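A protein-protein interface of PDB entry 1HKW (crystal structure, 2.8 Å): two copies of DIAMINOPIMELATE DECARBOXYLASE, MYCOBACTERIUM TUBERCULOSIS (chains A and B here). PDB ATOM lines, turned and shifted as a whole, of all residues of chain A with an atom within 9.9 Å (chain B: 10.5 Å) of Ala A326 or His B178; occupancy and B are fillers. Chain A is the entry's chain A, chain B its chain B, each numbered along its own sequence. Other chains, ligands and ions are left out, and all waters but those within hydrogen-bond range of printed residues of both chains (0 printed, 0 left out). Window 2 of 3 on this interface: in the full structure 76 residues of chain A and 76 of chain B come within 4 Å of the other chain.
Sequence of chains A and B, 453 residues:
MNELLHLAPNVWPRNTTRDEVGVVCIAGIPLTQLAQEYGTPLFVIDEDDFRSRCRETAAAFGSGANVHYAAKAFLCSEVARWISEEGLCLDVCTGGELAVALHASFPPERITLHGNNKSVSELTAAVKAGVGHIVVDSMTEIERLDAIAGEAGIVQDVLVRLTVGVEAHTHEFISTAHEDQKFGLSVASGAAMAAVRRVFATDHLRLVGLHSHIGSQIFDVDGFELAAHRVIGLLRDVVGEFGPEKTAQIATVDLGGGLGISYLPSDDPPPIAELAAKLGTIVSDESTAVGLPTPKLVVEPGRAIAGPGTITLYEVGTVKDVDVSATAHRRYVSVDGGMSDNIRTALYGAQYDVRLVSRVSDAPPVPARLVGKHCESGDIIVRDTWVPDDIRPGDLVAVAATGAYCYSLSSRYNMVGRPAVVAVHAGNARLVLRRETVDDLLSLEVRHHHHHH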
ATOM      1  N   VAL A 322      16.750 -13.495  18.379  1.00  0.00           N
ATOM      2  CA  VAL A 322      17.903 -12.723  17.869  1.00  0.00           C
ATOM      3  C   VAL A 322      18.991 -12.616  18.939  1.00  0.00           C
ATOM      4  O   VAL A 322      18.719 -12.236  20.090  1.00  0.00           O
ATOM      5  CB  VAL A 322      17.460 -11.314  17.402  1.00  0.00           C
ATOM      6  CG1 VAL A 322      18.646 -10.406  17.128  1.00  0.00           C
ATOM      7  CG2 VAL A 322      16.609 -11.433  16.174  1.00  0.00           C
ATOM      8  N   ASP A 323      20.225 -12.976  18.533  1.00  0.00           N
ATOM      9  CA  ASP A 323      21.393 -12.945  19.403  1.00  0.00           C
ATOM     10  C   ASP A 323      21.871 -11.487  19.542  1.00  0.00           C
ATOM     11  O   ASP A 323      22.150 -10.842  18.547  1.00  0.00           O
ATOM     12  CB  ASP A 323      22.518 -13.873  18.867  1.00  0.00           C
ATOM     13  CG  ASP A 323      22.809 -13.672  17.304  1.00  0.00           C
ATOM     14  OD1 ASP A 323      22.039 -14.249  16.428  1.00  0.00           O
ATOM     15  OD2 ASP A 323      23.806 -12.996  16.868  1.00  0.00           O
ATOM     16  N   VAL A 324      21.913 -10.991  20.794  1.00  0.00           N
ATOM     17  CA  VAL A 324      22.407  -9.624  21.141  1.00  0.00           C
ATOM     18  C   VAL A 324      23.713  -9.577  22.005  1.00  0.00           C
ATOM     19  O   VAL A 324      24.225  -8.481  22.276  1.00  0.00           O
ATOM     20  CB  VAL A 324      21.363  -8.825  21.939  1.00  0.00           C
ATOM     21  CG1 VAL A 324      20.086  -8.863  21.259  1.00  0.00           C
ATOM     22  CG2 VAL A 324      21.224  -9.373  23.405  1.00  0.00           C
ATOM     23  N   SER A 325      24.176 -10.745  22.496  1.00  0.00           N
ATOM     24  CA  SER A 325      25.502 -10.895  23.137  1.00  0.00           C
ATOM     25  C   SER A 325      25.944 -12.372  22.981  1.00  0.00           C
ATOM     26  O   SER A 325      25.329 -13.137  22.241  1.00  0.00           O
ATOM     27  CB  SER A 325      25.492 -10.430  24.609  1.00  0.00           C
ATOM     28  OG  SER A 325      24.750 -11.280  25.449  1.00  0.00           O
ATOM     29  N   ALA A 326      27.012 -12.765  23.633  1.00  0.00           N
ATOM     30  CA  ALA A 326      27.571 -14.104  23.400  1.00  0.00           C
ATOM     31  C   ALA A 326      26.660 -15.127  24.041  1.00  0.00           C
ATOM     32  O   ALA A 326      26.630 -16.316  23.690  1.00  0.00           O
ATOM     33  CB  ALA A 326      29.053 -14.210  24.015  1.00  0.00           C
ATOM     34  N   THR A 327      25.906 -14.637  24.962  1.00  0.00           N
ATOM     35  CA  THR A 327      25.273 -15.437  25.910  1.00  0.00           C
ATOM     36  C   THR A 327      23.727 -15.144  25.821  1.00  0.00           C
ATOM     37  O   THR A 327      22.941 -16.015  26.046  1.00  0.00           O
ATOM     38  CB  THR A 327      25.908 -15.114  27.374  1.00  0.00           C
ATOM     39  OG1 THR A 327      24.884 -15.016  28.340  1.00  0.00           O
ATOM     40  CG2 THR A 327      26.572 -13.662  27.468  1.00  0.00           C
ATOM     41  N   ALA A 328      23.321 -13.923  25.437  1.00  0.00           N
ATOM     42  CA  ALA A 328      21.894 -13.526  25.544  1.00  0.00           C
ATOM     43  C   ALA A 328      21.128 -13.360  24.185  1.00  0.00           C
ATOM     44  O   ALA A 328      21.736 -13.242  23.089  1.00  0.00           O
ATOM     45  CB  ALA A 328      21.765 -12.251  26.356  1.00  0.00           C
ATOM     46  N   HIS A 329      19.790 -13.325  24.307  1.00  0.00           N
ATOM     47  CA  HIS A 329      18.886 -13.261  23.171  1.00  0.00           C
ATOM     48  C   HIS A 329      17.773 -12.208  23.386  1.00  0.00           C
ATOM     49  O   HIS A 329      17.365 -11.915  24.528  1.00  0.00           O
ATOM     50  CB  HIS A 329      18.282 -14.670  22.894  1.00  0.00           C
ATOM     51  CG  HIS A 329      19.283 -15.642  22.340  1.00  0.00           C
ATOM     52  ND1 HIS A 329      20.036 -16.480  23.145  1.00  0.00           N
ATOM     53  CD2 HIS A 329      19.703 -15.865  21.061  1.00  0.00           C
ATOM     54  CE1 HIS A 329      20.856 -17.191  22.385  1.00  0.00           C
ATOM     55  NE2 HIS A 329      20.678 -16.827  21.117  1.00  0.00           N
ATOM     56  N   ARG A 330      17.300 -11.630  22.296  1.00  0.00           N
ATOM     57  CA  ARG A 330      16.090 -10.836  22.348  1.00  0.00           C
ATOM     58  C   ARG A 330      15.124 -11.437  21.425  1.00  0.00           C
ATOM     59  O   ARG A 330      15.465 -11.801  20.266  1.00  0.00           O
ATOM     60  CB  ARG A 330      16.345  -9.402  21.957  1.00  0.00           C
ATOM     61  CG  ARG A 330      15.219  -8.390  22.420  1.00  0.00           C
ATOM     62  CD  ARG A 330      15.438  -6.895  21.884  1.00  0.00           C
ATOM     63  NE  ARG A 330      16.846  -6.563  21.944  1.00  0.00           N
ATOM     64  CZ  ARG A 330      17.478  -6.259  23.056  1.00  0.00           C
ATOM     65  NH1 ARG A 330      16.826  -6.182  24.187  1.00  0.00           N
ATOM     66  NH2 ARG A 330      18.755  -6.004  23.036  1.00  0.00           N
ATOM     67  N   TYR A 332      12.207 -11.214  19.180  1.00  0.00           N
ATOM     68  CA  TYR A 332      11.479 -10.277  18.300  1.00  0.00           C
ATOM     69  C   TYR A 332      10.129 -10.871  17.887  1.00  0.00           C
ATOM     70  O   TYR A 332      10.065 -11.895  17.118  1.00  0.00           O
ATOM     71  CB  TYR A 332      12.318  -9.955  17.040  1.00  0.00           C
ATOM     72  CG  TYR A 332      13.314  -8.925  17.267  1.00  0.00           C
ATOM     73  CD1 TYR A 332      14.410  -9.190  18.023  1.00  0.00           C
ATOM     74  CD2 TYR A 332      13.159  -7.642  16.750  1.00  0.00           C
ATOM     75  CE1 TYR A 332      15.369  -8.212  18.253  1.00  0.00           C
ATOM     76  CE2 TYR A 332      14.122  -6.627  16.989  1.00  0.00           C
ATOM     77  CZ  TYR A 332      15.215  -6.918  17.728  1.00  0.00           C
ATOM     78  OH  TYR A 332      16.185  -5.963  17.999  1.00  0.00           O
ATOM     79  N   ARG A 369      11.152  -7.572  21.833  1.00  0.00           N
ATOM     80  CA  ARG A 369      10.766  -6.353  21.129  1.00  0.00           C
ATOM     81  C   ARG A 369       9.578  -6.651  20.305  1.00  0.00           C
ATOM     82  O   ARG A 369       9.582  -7.588  19.498  1.00  0.00           O
ATOM     83  CB  ARG A 369      11.888  -5.846  20.155  1.00  0.00           C
ATOM     84  CG  ARG A 369      12.702  -4.702  20.702  1.00  0.00           C
ATOM     85  CD  ARG A 369      13.108  -3.631  19.754  1.00  0.00           C
ATOM     86  NE  ARG A 369      14.588  -3.434  19.708  1.00  0.00           N
ATOM     87  CZ  ARG A 369      15.417  -3.222  20.765  1.00  0.00           C
ATOM     88  NH1 ARG A 369      14.985  -3.180  22.002  1.00  0.00           N
ATOM     89  NH2 ARG A 369      16.712  -3.077  20.548  1.00  0.00           N
ATOM     90  N   THR B 163      21.825 -10.766   8.472  1.00  0.00           N
ATOM     91  CA  THR B 163      22.557  -9.916   9.377  1.00  0.00           C
ATOM     92  C   THR B 163      24.087 -10.147   9.323  1.00  0.00           C
ATOM     93  O   THR B 163      24.582 -11.196   9.555  1.00  0.00           O
ATOM     94  CB  THR B 163      22.065 -10.258  10.715  1.00  0.00           C
ATOM     95  OG1 THR B 163      20.906  -9.516  10.951  1.00  0.00           O
ATOM     96  CG2 THR B 163      23.047  -9.818  11.872  1.00  0.00           C
ATOM     97  N   VAL B 164      24.820  -9.139   9.053  1.00  0.00           N
ATOM     98  CA  VAL B 164      26.228  -9.328   8.905  1.00  0.00           C
ATOM     99  C   VAL B 164      27.033  -8.377   9.859  1.00  0.00           C
ATOM    100  O   VAL B 164      28.268  -8.342   9.848  1.00  0.00           O
ATOM    101  CB  VAL B 164      26.543  -9.188   7.419  1.00  0.00           C
ATOM    102  CG1 VAL B 164      27.238  -7.865   7.078  1.00  0.00           C
ATOM    103  CG2 VAL B 164      27.312 -10.401   6.925  1.00  0.00           C
ATOM    104  N   GLY B 165      26.283  -7.660  10.706  1.00  0.00           N
ATOM    105  CA  GLY B 165      26.812  -6.765  11.706  1.00  0.00           C
ATOM    106  C   GLY B 165      27.464  -5.528  11.158  1.00  0.00           C
ATOM    107  O   GLY B 165      28.447  -5.105  11.717  1.00  0.00           O
ATOM    108  N   VAL B 166      26.920  -4.940  10.093  1.00  0.00           N
ATOM    109  CA  VAL B 166      27.396  -3.641   9.591  1.00  0.00           C
ATOM    110  C   VAL B 166      26.282  -2.603   9.508  1.00  0.00           C
ATOM    111  O   VAL B 166      25.252  -2.871   9.044  1.00  0.00           O
ATOM    112  CB  VAL B 166      28.015  -3.821   8.233  1.00  0.00           C
ATOM    113  CG1 VAL B 166      28.635  -2.477   7.695  1.00  0.00           C
ATOM    114  CG2 VAL B 166      29.043  -4.910   8.317  1.00  0.00           C
ATOM    115  N   GLU B 167      26.511  -1.415   9.979  1.00  0.00           N
ATOM    116  CA  GLU B 167      25.544  -0.334   9.785  1.00  0.00           C
ATOM    117  C   GLU B 167      26.253   0.910   9.275  1.00  0.00           C
ATOM    118  O   GLU B 167      27.021   1.466   9.956  1.00  0.00           O
ATOM    119  CB  GLU B 167      24.779  -0.003  11.093  1.00  0.00           C
ATOM    120  CG  GLU B 167      23.517   0.871  10.857  1.00  0.00           C
ATOM    121  CD  GLU B 167      22.695   1.178  12.116  1.00  0.00           C
ATOM    122  OE1 GLU B 167      22.805   0.483  13.149  1.00  0.00           O
ATOM    123  OE2 GLU B 167      21.922   2.118  12.062  1.00  0.00           O
ATOM    124  N   ILE B 174      29.395   1.176  11.686  1.00  0.00           N
ATOM    125  CA  ILE B 174      29.568   0.502  12.947  1.00  0.00           C
ATOM    126  C   ILE B 174      29.577  -0.999  12.701  1.00  0.00           C
ATOM    127  O   ILE B 174      28.767  -1.500  11.982  1.00  0.00           O
ATOM    128  CB  ILE B 174      28.438   0.916  13.934  1.00  0.00           C
ATOM    129  CG1 ILE B 174      28.297   2.418  13.939  1.00  0.00           C
ATOM    130  CG2 ILE B 174      28.764   0.469  15.359  1.00  0.00           C
ATOM    131  CD1 ILE B 174      27.914   3.073  15.363  1.00  0.00           C
ATOM    132  N   SER B 175      30.527  -1.713  13.269  1.00  0.00           N
ATOM    133  CA  SER B 175      30.498  -3.160  13.159  1.00  0.00           C
ATOM    134  C   SER B 175      30.127  -3.712  14.511  1.00  0.00           C
ATOM    135  O   SER B 175      30.457  -3.129  15.519  1.00  0.00           O
ATOM    136  CB  SER B 175      31.837  -3.709  12.680  1.00  0.00           C
ATOM    137  OG  SER B 175      31.867  -5.139  12.753  1.00  0.00           O
ATOM    138  N   THR B 176      29.423  -4.833  14.523  1.00  0.00           N
ATOM    139  CA  THR B 176      28.780  -5.284  15.740  1.00  0.00           C
ATOM    140  C   THR B 176      28.856  -6.695  15.814  1.00  0.00           C
ATOM    141  O   THR B 176      28.592  -7.390  14.830  1.00  0.00           O
ATOM    142  CB  THR B 176      27.367  -4.929  15.725  1.00  0.00           C
ATOM    143  OG1 THR B 176      27.249  -3.540  15.953  1.00  0.00           O
ATOM    144  CG2 THR B 176      26.688  -5.503  16.874  1.00  0.00           C
ATOM    145  N   ALA B 177      29.198  -7.170  16.992  1.00  0.00           N
ATOM    146  CA  ALA B 177      29.380  -8.577  17.175  1.00  0.00           C
ATOM    147  C   ALA B 177      28.029  -9.255  16.957  1.00  0.00           C
ATOM    148  O   ALA B 177      27.957 -10.324  16.327  1.00  0.00           O
ATOM    149  CB  ALA B 177      29.960  -8.883  18.581  1.00  0.00           C
ATOM    150  N   HIS B 178      26.969  -8.607  17.461  1.00  0.00           N
ATOM    151  CA  HIS B 178      25.631  -9.161  17.444  1.00  0.00           C
ATOM    152  C   HIS B 178      24.615  -8.082  17.085  1.00  0.00           C
ATOM    153  O   HIS B 178      24.183  -7.290  17.959  1.00  0.00           O
ATOM    154  CB  HIS B 178      25.267  -9.814  18.843  1.00  0.00           C
ATOM    155  CG  HIS B 178      26.226 -10.872  19.292  1.00  0.00           C
ATOM    156  ND1 HIS B 178      26.510 -11.995  18.534  1.00  0.00           N
ATOM    157  CD2 HIS B 178      26.999 -10.960  20.399  1.00  0.00           C
ATOM    158  CE1 HIS B 178      27.417 -12.728  19.154  1.00  0.00           C
ATOM    159  NE2 HIS B 178      27.717 -12.134  20.301  1.00  0.00           N
ATOM    160  N   GLU B 179      24.215  -8.042  15.812  1.00  0.00           N
ATOM    161  CA  GLU B 179      23.275  -7.026  15.359  1.00  0.00           C
ATOM    162  C   GLU B 179      21.885  -7.328  15.977  1.00  0.00           C
ATOM    163  O   GLU B 179      21.456  -8.508  16.056  1.00  0.00           O
ATOM    164  CB  GLU B 179      23.206  -6.965  13.816  1.00  0.00           C
ATOM    165  CG  GLU B 179      22.873  -5.544  13.256  1.00  0.00           C
ATOM    166  CD  GLU B 179      22.790  -5.491  11.707  1.00  0.00           C
ATOM    167  OE1 GLU B 179      22.973  -6.552  11.004  1.00  0.00           O
ATOM    168  OE2 GLU B 179      22.545  -4.378  11.195  1.00  0.00           O
ATOM    169  N   ASP B 180      21.200  -6.263  16.403  1.00  0.00           N
ATOM    170  CA  ASP B 180      20.115  -6.356  17.339  1.00  0.00           C
ATOM    171  C   ASP B 180      18.895  -5.610  16.764  1.00  0.00           C
ATOM    172  O   ASP B 180      18.572  -4.461  17.122  1.00  0.00           O
ATOM    173  CB  ASP B 180      20.546  -5.809  18.692  1.00  0.00           C
ATOM    174  CG  ASP B 180      19.462  -5.908  19.717  1.00  0.00           C
ATOM    175  OD1 ASP B 180      19.588  -5.275  20.766  1.00  0.00           O
ATOM    176  OD2 ASP B 180      18.407  -6.574  19.554  1.00  0.00           O
ATOM    177  N   GLN B 181      18.223  -6.300  15.865  1.00  0.00           N
ATOM    178  CA  GLN B 181      17.194  -5.722  15.030  1.00  0.00           C
ATOM    179  C   GLN B 181      16.407  -6.848  14.320  1.00  0.00           C
ATOM    180  O   GLN B 181      16.791  -8.004  14.341  1.00  0.00           O
ATOM    181  CB  GLN B 181      17.833  -4.806  14.001  1.00  0.00           C
ATOM    182  CG  GLN B 181      18.769  -5.575  12.987  1.00  0.00           C
ATOM    183  CD  GLN B 181      18.194  -5.618  11.619  1.00  0.00           C
ATOM    184  OE1 GLN B 181      18.885  -5.761  10.668  1.00  0.00           O
ATOM    185  NE2 GLN B 181      16.937  -5.465  11.534  1.00  0.00           N
ATOM    186  N   LYS B 182      15.328  -6.487  13.654  1.00  0.00           N
ATOM    187  CA  LYS B 182      14.310  -7.463  13.332  1.00  0.00           C
ATOM    188  C   LYS B 182      14.616  -8.334  12.097  1.00  0.00           C
ATOM    189  O   LYS B 182      14.223  -9.493  12.074  1.00  0.00           O
ATOM    190  CB  LYS B 182      12.934  -6.794  13.246  1.00  0.00           C
ATOM    191  CG  LYS B 182      12.637  -6.040  11.964  1.00  0.00           C
ATOM    192  CD  LYS B 182      11.290  -5.260  12.116  1.00  0.00           C
ATOM    193  CE  LYS B 182      10.912  -4.521  10.868  1.00  0.00           C
ATOM    194  NZ  LYS B 182       9.438  -4.113  10.877  1.00  0.00           N
ATOM    195  N   PHE B 183      15.326  -7.800  11.108  1.00  0.00           N
ATOM    196  CA  PHE B 183      15.543  -8.514   9.855  1.00  0.00           C
ATOM    197  C   PHE B 183      16.661  -9.525   9.919  1.00  0.00           C
ATOM    198  O   PHE B 183      17.637  -9.383  10.665  1.00  0.00           O
ATOM    199  CB  PHE B 183      15.906  -7.537   8.733  1.00  0.00           C
ATOM    200  CG  PHE B 183      14.826  -6.644   8.374  1.00  0.00           C
ATOM    201  CD1 PHE B 183      13.686  -7.139   7.720  1.00  0.00           C
ATOM    202  CD2 PHE B 183      14.894  -5.299   8.705  1.00  0.00           C
ATOM    203  CE1 PHE B 183      12.633  -6.292   7.395  1.00  0.00           C
ATOM    204  CE2 PHE B 183      13.879  -4.461   8.403  1.00  0.00           C
ATOM    205  CZ  PHE B 183      12.720  -4.949   7.739  1.00  0.00           C
ATOM    206  N   LEU B 185      18.932 -13.242   9.140  1.00  0.00           N
ATOM    207  CA  LEU B 185      19.425 -14.283   9.992  1.00  0.00           C
ATOM    208  C   LEU B 185      20.922 -14.131  10.139  1.00  0.00           C
ATOM    209  O   LEU B 185      21.640 -13.873   9.163  1.00  0.00           O
ATOM    210  CB  LEU B 185      19.075 -15.641   9.419  1.00  0.00           C
ATOM    211  CG  LEU B 185      17.586 -15.977   9.470  1.00  0.00           C
ATOM    212  CD1 LEU B 185      17.289 -16.859   8.345  1.00  0.00           C
ATOM    213  CD2 LEU B 185      17.135 -16.635  10.810  1.00  0.00           C
ATOM    214  N   SER B 186      21.385 -14.299  11.372  1.00  0.00           N
ATOM    215  CA  SER B 186      22.773 -14.032  11.687  1.00  0.00           C
ATOM    216  C   SER B 186      23.719 -15.092  11.046  1.00  0.00           C
ATOM    217  O   SER B 186      23.474 -16.290  11.117  1.00  0.00           O
ATOM    218  CB  SER B 186      22.965 -13.960  13.192  1.00  0.00           C
ATOM    219  OG  SER B 186      24.310 -14.086  13.509  1.00  0.00           O
ATOM    220  N   VAL B 187      24.767 -14.625  10.391  1.00  0.00           N
ATOM    221  CA  VAL B 187      25.854 -15.492   9.916  1.00  0.00           C
ATOM    222  C   VAL B 187      26.649 -16.098  11.080  1.00  0.00           C
ATOM    223  O   VAL B 187      27.020 -17.240  11.046  1.00  0.00           O
ATOM    224  CB  VAL B 187      26.872 -14.691   9.079  1.00  0.00           C
ATOM    225  CG1 VAL B 187      28.080 -15.572   8.720  1.00  0.00           C
ATOM    226  CG2 VAL B 187      26.218 -14.118   7.823  1.00  0.00           C
ATOM    227  N   ALA B 188      26.935 -15.290  12.084  1.00  0.00           N
ATOM    228  CA  ALA B 188      27.877 -15.682  13.101  1.00  0.00           C
ATOM    229  C   ALA B 188      27.258 -16.756  14.024  1.00  0.00           C
ATOM    230  O   ALA B 188      27.941 -17.635  14.482  1.00  0.00           O
ATOM    231  CB  ALA B 188      28.331 -14.452  13.914  1.00  0.00           C
ATOM    232  N   SER B 189      25.962 -16.683  14.274  1.00  0.00           N
ATOM    233  CA  SER B 189      25.326 -17.702  15.082  1.00  0.00           C
ATOM    234  C   SER B 189      25.104 -18.969  14.256  1.00  0.00           C
ATOM    235  O   SER B 189      24.668 -19.954  14.759  1.00  0.00           O
ATOM    236  CB  SER B 189      23.990 -17.182  15.636  1.00  0.00           C
ATOM    237  OG  SER B 189      23.004 -17.010  14.611  1.00  0.00           O
ATOM    238  N   GLY B 190      25.383 -18.883  12.963  1.00  0.00           N
ATOM    239  CA  GLY B 190      25.098 -19.951  12.024  1.00  0.00           C
ATOM    240  C   GLY B 190      23.614 -20.143  11.682  1.00  0.00           C
ATOM    241  O   GLY B 190      23.272 -21.111  10.979  1.00  0.00           O
ATOM    242  N   ALA B 191      22.726 -19.234  12.159  1.00  0.00           N
ATOM    243  CA  ALA B 191      21.299 -19.247  11.734  1.00  0.00           C
ATOM    244  C   ALA B 191      21.164 -19.103  10.205  1.00  0.00           C
ATOM    245  O   ALA B 191      20.295 -19.759   9.572  1.00  0.00           O
ATOM    246  CB  ALA B 191      20.579 -18.193  12.376  1.00  0.00           C
ATOM    247  N   ARG B 230      31.970 -10.269   4.542  1.00  0.00           N
ATOM    248  CA  ARG B 230      31.267 -11.076   5.473  1.00  0.00           C
ATOM    249  C   ARG B 230      30.148 -11.945   4.846  1.00  0.00           C
ATOM    250  O   ARG B 230      29.842 -13.056   5.350  1.00  0.00           O
ATOM    251  CB  ARG B 230      30.660 -10.173   6.515  1.00  0.00           C
ATOM    252  CG  ARG B 230      31.287 -10.242   7.868  1.00  0.00           C
ATOM    253  CD  ARG B 230      32.016  -8.984   8.298  1.00  0.00           C
ATOM    254  NE  ARG B 230      31.233  -8.290   9.280  1.00  0.00           N
ATOM    255  CZ  ARG B 230      31.738  -7.620  10.292  1.00  0.00           C
ATOM    256  NH1 ARG B 230      30.940  -7.029  11.121  1.00  0.00           N
ATOM    257  NH2 ARG B 230      33.035  -7.509  10.467  1.00  0.00           N
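The backbone NH of Ala B191 sits close to the side-chain hydroxyl of Ser B189, at 3.3 Å.
NE of Arg A369 is in hydrogen-bond range of OH of Tyr A332.
N of Ala A328 is in hydrogen-bond range of OG of Ser A325.
N of Ala B191 lies within hydrogen-bond range of O of Ser B186, at 3.2 Å.
The backbone NH (N) of Phe B183 sits close to the side-chain amide nitrogen (NE2) of Gln B181, at 2.9 Å.
N of Arg A330 sits at hydrogen-bond distance from O of Val A322 (2.7 Å).
Val A322 touches Glu B179 (CG1 to O, 3.6 Å).
Gln B181 touches Val A322 (O to CG2, 3.9 Å).
Asp A323 touches Ser B186 (OD1 to CB, 3.4 Å).
Val A324 touches His B178 (C to CB, 3.5 Å).
OD2 of Asp B180 touches CG1 of Val A324 (3.3 Å).
Tyr A332 touches Lys B182 (CE2 to N, 3.5 Å).
No position is printed for both chains.
Hydrophobic or aromatic side chains of chain B that line the printed part of chain A: His B178.
Of the 11 printed residues of chain A, 8 touch a printed residue of chain B.
Hydrophobic or aromatic side chains of chain A within 4 Å of the printed part of chain B: Val A322, Val A324 and Tyr A332.
Along chain A the printed residues that touch a printed residue of chain B span positions 322 to 369.
Among the printed residues, 15 pairs touch across the chains.
Among the printed residues, Asp or Glu carboxylates within 4 Å of a Lys or Arg side-chain nitrogen of the other chain: Arg A330 with Asp B180 (2.5 Å) and Arg A369 with Asp B180 (3.6 Å).
Of chain B, only His B178 comes within 4 Å of Ala A326.
Of chain A, only Asp A323 (3.3 Å), Val A324 (3.5 Å), Ser A325 (3.1 Å) and Ala A326 (3.5 Å) come within 4 Å of His B178.
Asp A323 touches just these residues of chain B: His B178, Glu B179, Ser B186 and Ser B189.
Val A324 touches just these residues of chain B: His B178 and Asp B180.
Ser A325 touches just one residue of chain B: His B178 (3.1 Å).
No residue of chain B comes within 4 Å of Thr A327.
No residue of chain B comes within 4 Å of Ala A328.
No residue of chain A comes within 4 Å of Ala B177.
Of the printed residues of chain A, Lys B182 touches Tyr A332 (3.5 Å).
Printed residues of chain A within 4 Å of Asp B180: Val A324, Arg A330, Tyr A332 and Arg A369.
The nearest residue of chain B that does not touch Ala A326 is Ala B177 (7.0 Å).
The nearest residue of chain A that does not touch His B178 is Thr A327 (5.6 Å).
The side-chain hydroxyl (OG) of Ser B189 lies within hydrogen-bond range of the side-chain carboxylate (OD1) of Asp A323.
The backbone carbonyl oxygen of Asp A323 lies close to the backbone carbonyl oxygen of Glu B179, at 3.5 Å.
The backbone carbonyl oxygen (O) of Ser A325 lies close to a ring nitrogen (NE2) of His B178 (3.2 Å).
N of Gln B181 is in hydrogen-bond range of OH of Tyr A332, at 3.0 Å.
The side-chain carboxylate of Asp B180 lies within salt-bridge range of the guanidinium group of Arg A330 (2.5 Å).
The side-chain hydroxyl of Tyr A332 is in hydrogen-bond range of the side-chain carboxylate of Asp B180 (2.8 Å).
The guanidinium group (NH2) of Arg A369 is in salt-bridge range of the side-chain carboxylate (OD1) of Asp B180 (3.6 Å).
A ring nitrogen (NE2) of His B178 lies within hydrogen-bond range of the backbone NH of Ala A326, 3.5 Å away.
The side-chain carboxylate (OD2) of Asp A323 is in hydrogen-bond range of a ring nitrogen (ND1) of His B178 (3.3 Å).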
